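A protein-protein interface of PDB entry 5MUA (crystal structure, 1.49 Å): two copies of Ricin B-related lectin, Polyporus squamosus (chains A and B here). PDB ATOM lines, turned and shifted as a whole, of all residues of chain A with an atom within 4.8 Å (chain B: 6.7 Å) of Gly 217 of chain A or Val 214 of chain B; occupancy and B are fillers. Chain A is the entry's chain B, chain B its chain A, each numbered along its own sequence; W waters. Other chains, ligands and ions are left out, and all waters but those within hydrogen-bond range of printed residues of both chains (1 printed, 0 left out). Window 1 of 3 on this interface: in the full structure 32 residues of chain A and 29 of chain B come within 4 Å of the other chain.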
ATOM      1  N   THR A 213       8.115 -14.838 -18.545  1.00  0.00           N
ATOM      2  CA  THR A 213       8.494 -13.480 -18.117  1.00  0.00           C
ATOM      3  C   THR A 213       9.684 -13.528 -17.193  1.00  0.00           C
ATOM      4  O   THR A 213      10.572 -12.696 -17.317  1.00  0.00           O
ATOM      5  CB  THR A 213       7.298 -12.778 -17.431  1.00  0.00           C
ATOM      6  OG1 THR A 213       6.307 -12.598 -18.400  1.00  0.00           O
ATOM      7  CG2 THR A 213       7.689 -11.364 -16.904  1.00  0.00           C
ATOM      8  N   VAL A 214       9.702 -14.441 -16.223  1.00  0.00           N
ATOM      9  CA  VAL A 214      10.770 -14.545 -15.281  1.00  0.00           C
ATOM     10  C   VAL A 214      12.064 -14.947 -16.046  1.00  0.00           C
ATOM     11  O   VAL A 214      13.116 -14.388 -15.750  1.00  0.00           O
ATOM     12  CB  VAL A 214      10.472 -15.514 -14.102  1.00  0.00           C
ATOM     13  CG1 VAL A 214      11.706 -15.791 -13.260  1.00  0.00           C
ATOM     14  CG2 VAL A 214       9.388 -14.904 -13.215  1.00  0.00           C
ATOM     15  N   PHE A 215      11.969 -15.910 -16.960  1.00  0.00           N
ATOM     16  CA  PHE A 215      13.176 -16.299 -17.721  1.00  0.00           C
ATOM     17  C   PHE A 215      13.750 -15.097 -18.486  1.00  0.00           C
ATOM     18  O   PHE A 215      14.997 -14.887 -18.444  1.00  0.00           O
ATOM     19  CB  PHE A 215      12.968 -17.520 -18.622  1.00  0.00           C
ATOM     20  CG  PHE A 215      14.230 -17.961 -19.305  1.00  0.00           C
ATOM     21  CD1 PHE A 215      15.331 -18.282 -18.536  1.00  0.00           C
ATOM     22  CD2 PHE A 215      14.316 -17.996 -20.688  1.00  0.00           C
ATOM     23  CE1 PHE A 215      16.536 -18.655 -19.137  1.00  0.00           C
ATOM     24  CE2 PHE A 215      15.513 -18.329 -21.295  1.00  0.00           C
ATOM     25  CZ  PHE A 215      16.580 -18.716 -20.500  1.00  0.00           C
ATOM     26  N   LYS A 216      12.873 -14.334 -19.128  1.00  0.00           N
ATOM     27  CA  LYS A 216      13.283 -13.135 -19.815  1.00  0.00           C
ATOM     28  C   LYS A 216      14.045 -12.175 -18.934  1.00  0.00           C
ATOM     29  O   LYS A 216      15.107 -11.577 -19.335  1.00  0.00           O
ATOM     30  CB  LYS A 216      12.165 -12.498 -20.618  1.00  0.00           C
ATOM     31  CG  LYS A 216      12.575 -11.239 -21.340  1.00  0.00           C
ATOM     32  CD  LYS A 216      11.574 -10.752 -22.367  1.00  0.00           C
ATOM     33  CE  LYS A 216      12.003  -9.365 -22.856  1.00  0.00           C
ATOM     34  NZ  LYS A 216      13.351  -9.369 -23.490  1.00  0.00           N
ATOM     35  N   GLY A 217      13.526 -12.002 -17.731  1.00  0.00           N
ATOM     36  CA  GLY A 217      14.280 -11.221 -16.736  1.00  0.00           C
ATOM     37  C   GLY A 217      15.583 -11.821 -16.268  1.00  0.00           C
ATOM     38  O   GLY A 217      16.615 -11.078 -16.018  1.00  0.00           O
ATOM     39  N   ALA A 218      15.608 -13.146 -16.148  1.00  0.00           N
ATOM     40  CA  ALA A 218      16.862 -13.849 -15.814  1.00  0.00           C
ATOM     41  C   ALA A 218      17.979 -13.561 -16.832  1.00  0.00           C
ATOM     42  O   ALA A 218      19.118 -13.385 -16.462  1.00  0.00           O
ATOM     43  CB  ALA A 218      16.636 -15.357 -15.676  1.00  0.00           C
ATOM     44  N   VAL A 219      17.606 -13.523 -18.110  1.00  0.00           N
ATOM     45  CA  VAL A 219      18.584 -13.299 -19.197  1.00  0.00           C
ATOM     46  C   VAL A 219      19.045 -11.864 -19.040  1.00  0.00           C
ATOM     47  O   VAL A 219      20.262 -11.632 -19.078  1.00  0.00           O
ATOM     48  CB  VAL A 219      18.002 -13.551 -20.580  1.00  0.00           C
ATOM     49  CG1 VAL A 219      19.034 -13.191 -21.646  1.00  0.00           C
ATOM     50  CG2 VAL A 219      17.683 -15.034 -20.683  1.00  0.00           C
ATOM     51  N   ALA A 220      18.108 -10.948 -18.793  1.00  0.00           N
ATOM     52  CA  ALA A 220      18.502  -9.524 -18.660  1.00  0.00           C
ATOM     53  C   ALA A 220      19.501  -9.343 -17.470  1.00  0.00           C
ATOM     54  O   ALA A 220      20.478  -8.620 -17.567  1.00  0.00           O
ATOM     55  CB  ALA A 220      17.282  -8.652 -18.485  1.00  0.00           C
ATOM     56  N   LYS A 221      19.230  -9.964 -16.323  1.00  0.00           N
ATOM     57  CA  LYS A 221      20.125  -9.846 -15.173  1.00  0.00           C
ATOM     58  C   LYS A 221      21.453 -10.497 -15.469  1.00  0.00           C
ATOM     59  O   LYS A 221      22.483  -9.961 -15.083  1.00  0.00           O
ATOM     60  CB  LYS A 221      19.509 -10.420 -13.864  1.00  0.00           C
ATOM     61  CG  LYS A 221      18.215  -9.708 -13.428  1.00  0.00           C
ATOM     62  CD  LYS A 221      17.652 -10.298 -12.128  1.00  0.00           C
ATOM     63  CE  LYS A 221      18.553  -9.921 -10.953  1.00  0.00           C
ATOM     64  NZ  LYS A 221      18.009 -10.102  -9.572  1.00  0.00           N
ATOM     65  N   SER B 194      14.245  -6.359  -4.405  1.00  0.00           N
ATOM     66  CA  SER B 194      14.596  -6.698  -5.805  1.00  0.00           C
ATOM     67  C   SER B 194      16.039  -6.370  -6.112  1.00  0.00           C
ATOM     68  O   SER B 194      16.616  -6.957  -7.040  1.00  0.00           O
ATOM     69  CB  SER B 194      13.777  -5.894  -6.793  1.00  0.00           C
ATOM     70  OG  SER B 194      14.131  -4.540  -6.859  1.00  0.00           O
ATOM     71  N   LEU B 196      16.801  -3.561  -7.399  1.00  0.00           N
ATOM     72  CA  LEU B 196      16.811  -2.664  -8.563  1.00  0.00           C
ATOM     73  C   LEU B 196      17.216  -1.257  -8.229  1.00  0.00           C
ATOM     74  O   LEU B 196      17.826  -0.583  -9.033  1.00  0.00           O
ATOM     75  CB  LEU B 196      15.483  -2.659  -9.329  1.00  0.00           C
ATOM     76  CG  LEU B 196      15.090  -3.998  -9.953  1.00  0.00           C
ATOM     77  CD1 LEU B 196      13.643  -4.000 -10.316  1.00  0.00           C
ATOM     78  CD2 LEU B 196      15.951  -4.208 -11.204  1.00  0.00           C
ATOM     79  N   PHE B 206      21.120  -2.533 -19.422  1.00  0.00           N
ATOM     80  CA  PHE B 206      20.157  -2.591 -18.280  1.00  0.00           C
ATOM     81  C   PHE B 206      19.526  -1.229 -18.147  1.00  0.00           C
ATOM     82  O   PHE B 206      19.899  -0.445 -17.310  1.00  0.00           O
ATOM     83  CB  PHE B 206      20.837  -3.011 -17.003  1.00  0.00           C
ATOM     84  CG  PHE B 206      19.895  -3.684 -16.079  1.00  0.00           C
ATOM     85  CD1 PHE B 206      19.545  -5.015 -16.278  1.00  0.00           C
ATOM     86  CD2 PHE B 206      19.270  -2.974 -15.123  1.00  0.00           C
ATOM     87  CE1 PHE B 206      18.630  -5.644 -15.416  1.00  0.00           C
ATOM     88  CE2 PHE B 206      18.358  -3.586 -14.253  1.00  0.00           C
ATOM     89  CZ  PHE B 206      18.040  -4.906 -14.389  1.00  0.00           C
ATOM     90  N   ASP B 209      13.572  -0.770 -20.125  1.00  0.00           N
ATOM     91  CA  ASP B 209      12.889  -2.015 -20.420  1.00  0.00           C
ATOM     92  C   ASP B 209      13.273  -3.133 -19.468  1.00  0.00           C
ATOM     93  O   ASP B 209      12.454  -3.901 -19.079  1.00  0.00           O
ATOM     94  CB  ASP B 209      13.030  -2.390 -21.880  1.00  0.00           C
ATOM     95  CG  ASP B 209      14.463  -2.436 -22.348  1.00  0.00           C
ATOM     96  OD1 ASP B 209      15.073  -3.493 -22.232  1.00  0.00           O
ATOM     97  OD2 ASP B 209      14.920  -1.365 -22.805  1.00  0.00           O
ATOM     98  N   ASP B 210      14.555  -3.182 -19.089  1.00  0.00           N
ATOM     99  CA  ASP B 210      15.034  -4.156 -18.156  1.00  0.00           C
ATOM    100  C   ASP B 210      14.488  -3.933 -16.755  1.00  0.00           C
ATOM    101  O   ASP B 210      14.100  -4.874 -16.126  1.00  0.00           O
ATOM    102  CB  ASP B 210      16.557  -4.169 -18.147  1.00  0.00           C
ATOM    103  CG  ASP B 210      17.093  -4.525 -19.539  1.00  0.00           C
ATOM    104  OD1 ASP B 210      16.852  -5.661 -19.983  1.00  0.00           O
ATOM    105  OD2 ASP B 210      17.627  -3.671 -20.180  1.00  0.00           O
ATOM    106  N   PHE B 211      14.524  -2.689 -16.265  1.00  0.00           N
ATOM    107  CA  PHE B 211      13.989  -2.450 -14.933  1.00  0.00           C
ATOM    108  C   PHE B 211      12.517  -2.909 -14.838  1.00  0.00           C
ATOM    109  O   PHE B 211      12.120  -3.592 -13.861  1.00  0.00           O
ATOM    110  CB  PHE B 211      14.159  -0.965 -14.507  1.00  0.00           C
ATOM    111  CG  PHE B 211      15.553  -0.599 -14.120  1.00  0.00           C
ATOM    112  CD1 PHE B 211      16.453  -0.146 -15.092  1.00  0.00           C
ATOM    113  CD2 PHE B 211      15.970  -0.613 -12.775  1.00  0.00           C
ATOM    114  CE1 PHE B 211      17.741   0.242 -14.739  1.00  0.00           C
ATOM    115  CE2 PHE B 211      17.249  -0.229 -12.419  1.00  0.00           C
ATOM    116  CZ  PHE B 211      18.143   0.199 -13.421  1.00  0.00           C
ATOM    117  N   ALA B 212      11.751  -2.581 -15.874  1.00  0.00           N
ATOM    118  CA  ALA B 212      10.310  -2.815 -15.848  1.00  0.00           C
ATOM    119  C   ALA B 212      10.005  -4.324 -16.003  1.00  0.00           C
ATOM    120  O   ALA B 212       9.162  -4.870 -15.310  1.00  0.00           O
ATOM    121  CB  ALA B 212       9.660  -1.991 -16.919  1.00  0.00           C
ATOM    122  N   THR B 213      10.736  -4.984 -16.885  1.00  0.00           N
ATOM    123  CA  THR B 213      10.591  -6.425 -17.067  1.00  0.00           C
ATOM    124  C   THR B 213      11.051  -7.207 -15.840  1.00  0.00           C
ATOM    125  O   THR B 213      10.373  -8.108 -15.437  1.00  0.00           O
ATOM    126  CB  THR B 213      11.381  -6.914 -18.366  1.00  0.00           C
ATOM    127  OG1 THR B 213      10.783  -6.293 -19.507  1.00  0.00           O
ATOM    128  CG2 THR B 213      11.218  -8.391 -18.557  1.00  0.00           C
ATOM    129  N   VAL B 214      12.234  -6.909 -15.313  1.00  0.00           N
ATOM    130  CA  VAL B 214      12.780  -7.566 -14.137  1.00  0.00           C
ATOM    131  C   VAL B 214      11.839  -7.378 -12.939  1.00  0.00           C
ATOM    132  O   VAL B 214      11.528  -8.308 -12.285  1.00  0.00           O
ATOM    133  CB  VAL B 214      14.223  -7.146 -13.873  1.00  0.00           C
ATOM    134  CG1 VAL B 214      14.730  -7.609 -12.528  1.00  0.00           C
ATOM    135  CG2 VAL B 214      15.101  -7.745 -14.957  1.00  0.00           C
ATOM    136  N   PHE B 215      11.365  -6.158 -12.753  1.00  0.00           N
ATOM    137  CA  PHE B 215      10.478  -5.893 -11.608  1.00  0.00           C
ATOM    138  C   PHE B 215       9.165  -6.710 -11.755  1.00  0.00           C
ATOM    139  O   PHE B 215       8.732  -7.320 -10.778  1.00  0.00           O
ATOM    140  CB  PHE B 215      10.209  -4.378 -11.384  1.00  0.00           C
ATOM    141  CG  PHE B 215       9.379  -4.144 -10.163  1.00  0.00           C
ATOM    142  CD1 PHE B 215       9.857  -4.577  -8.903  1.00  0.00           C
ATOM    143  CD2 PHE B 215       8.083  -3.650 -10.283  1.00  0.00           C
ATOM    144  CE1 PHE B 215       9.069  -4.452  -7.761  1.00  0.00           C
ATOM    145  CE2 PHE B 215       7.292  -3.500  -9.145  1.00  0.00           C
ATOM    146  CZ  PHE B 215       7.813  -3.885  -7.888  1.00  0.00           C
ATOM    147  N   LYS B 216       8.599  -6.786 -12.951  1.00  0.00           N
ATOM    148  CA  LYS B 216       7.359  -7.603 -13.119  1.00  0.00           C
ATOM    149  C   LYS B 216       7.647  -9.018 -12.755  1.00  0.00           C
ATOM    150  O   LYS B 216       6.858  -9.662 -12.100  1.00  0.00           O
ATOM    151  CB  LYS B 216       6.814  -7.413 -14.527  1.00  0.00           C
ATOM    152  CG  LYS B 216       5.561  -8.218 -14.786  1.00  0.00           C
ATOM    153  CD  LYS B 216       4.900  -7.910 -16.086  1.00  0.00           C
ATOM    154  CE  LYS B 216       3.778  -8.902 -16.371  1.00  0.00           C
ATOM    155  NZ  LYS B 216       2.875  -9.102 -15.190  1.00  0.00           N
ATOM    156  N   GLY B 217       8.800  -9.523 -13.185  1.00  0.00           N
ATOM    157  CA  GLY B 217       9.216 -10.848 -12.756  1.00  0.00           C
ATOM    158  C   GLY B 217       9.444 -11.005 -11.266  1.00  0.00           C
ATOM    159  O   GLY B 217       9.157 -12.069 -10.701  1.00  0.00           O
ATOM    160  N   ALA B 218       9.988  -9.969 -10.624  1.00  0.00           N
ATOM    161  CA  ALA B 218      10.159 -10.013  -9.180  1.00  0.00           C
ATOM    162  C   ALA B 218       8.823 -10.158  -8.456  1.00  0.00           C
ATOM    163  O   ALA B 218       8.706 -10.923  -7.488  1.00  0.00           O
ATOM    164  CB  ALA B 218      10.914  -8.810  -8.701  1.00  0.00           C
ATOM    165  N   VAL B 219       7.794  -9.470  -8.959  1.00  0.00           N
ATOM    166  CA  VAL B 219       6.506  -9.577  -8.315  1.00  0.00           C
ATOM    167  C   VAL B 219       5.975 -11.047  -8.461  1.00  0.00           C
ATOM    168  O   VAL B 219       5.472 -11.632  -7.501  1.00  0.00           O
ATOM    169  CB  VAL B 219       5.508  -8.566  -8.875  1.00  0.00           C
ATOM    170  CG1 VAL B 219       4.115  -8.880  -8.340  1.00  0.00           C
ATOM    171  CG2 VAL B 219       5.924  -7.196  -8.511  1.00  0.00           C
ATOM    172  N   LYS B 221       7.729 -13.803  -8.805  1.00  0.00           N
ATOM    173  CA  LYS B 221       8.473 -14.723  -7.954  1.00  0.00           C
ATOM    174  C   LYS B 221       8.059 -14.607  -6.486  1.00  0.00           C
ATOM    175  O   LYS B 221       8.019 -15.589  -5.743  1.00  0.00           O
ATOM    176  CB  LYS B 221       9.968 -14.511  -8.084  1.00  0.00           C
ATOM    177  CG  LYS B 221      10.502 -15.031  -9.402  1.00  0.00           C
ATOM    178  CD  LYS B 221      12.032 -15.120  -9.421  1.00  0.00           C
ATOM    179  CE  LYS B 221      12.670 -13.830  -8.949  1.00  0.00           C
ATOM    180  NZ  LYS B 221      14.095 -13.856  -9.249  1.00  0.00           N
HETATM  181  O   HOH W   1      11.300 -10.846 -15.297  1.00  0.00           O
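O of Gly 217 of chain B touches CG2 of Val 214 of chain A, 3.8 Å away. Val 214 of chain A touches Lys 221 of chain B. Val 214 of chain B touches Gly 217 of chain A. Ala 220 of chain A touches Phe 206 of chain B (O to CD1, 3.9 Å). Asp 210 of chain B touches Ala 220 of chain A (OD1 to CB, 3.4 Å). Lys 221 of chain A touches Val 214 of chain B.
Printed residues of chain B within 4 Å of Val 214 of chain A: Gly 217 and Lys 221. Of the printed residues of chain B, Ala 220 of chain A touches Phe 206 (3.9 Å) and Asp 210 (3.4 Å). Of the printed residues of chain A, Phe 206 of chain B touches Ala 220. Of the printed residues of chain A, Asp 210 of chain B touches Ala 220. Thr 213 of chain B touches none of the printed residues of chain A. Printed residues of chain A within 4 Å of Val 214 of chain B: Gly 217 and Lys 221. Of the printed residues of chain A, Gly 217 of chain B touches Val 214 (3.8 Å). The nearest residue of chain B that does not touch Gly 217 of chain A is Thr 213 of chain B (4.4 Å).
Hydrophobic or aromatic side chains of chain A that line the printed part of chain B: Val 214 and Ala 220.
Val 214 of chain A touches Gly 217 of chain B, and with the chains exchanged Gly 217 of chain A touches Val 214 of chain B. Val 214 of chain A touches Lys 221 of chain B, and with the chains exchanged Lys 221 of chain A touches Val 214 of chain B. 8 positions are printed for both chains.
Water W1 lies within hydrogen-bond range of the backbone carbonyl oxygen (O) of Thr 213 of chain A (2.8 Å), the backbone carbonyl oxygen (O) of Thr 213 of chain B (2.9 Å) and the backbone NH (N) of Gly 217 of chain A (3.5 Å).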
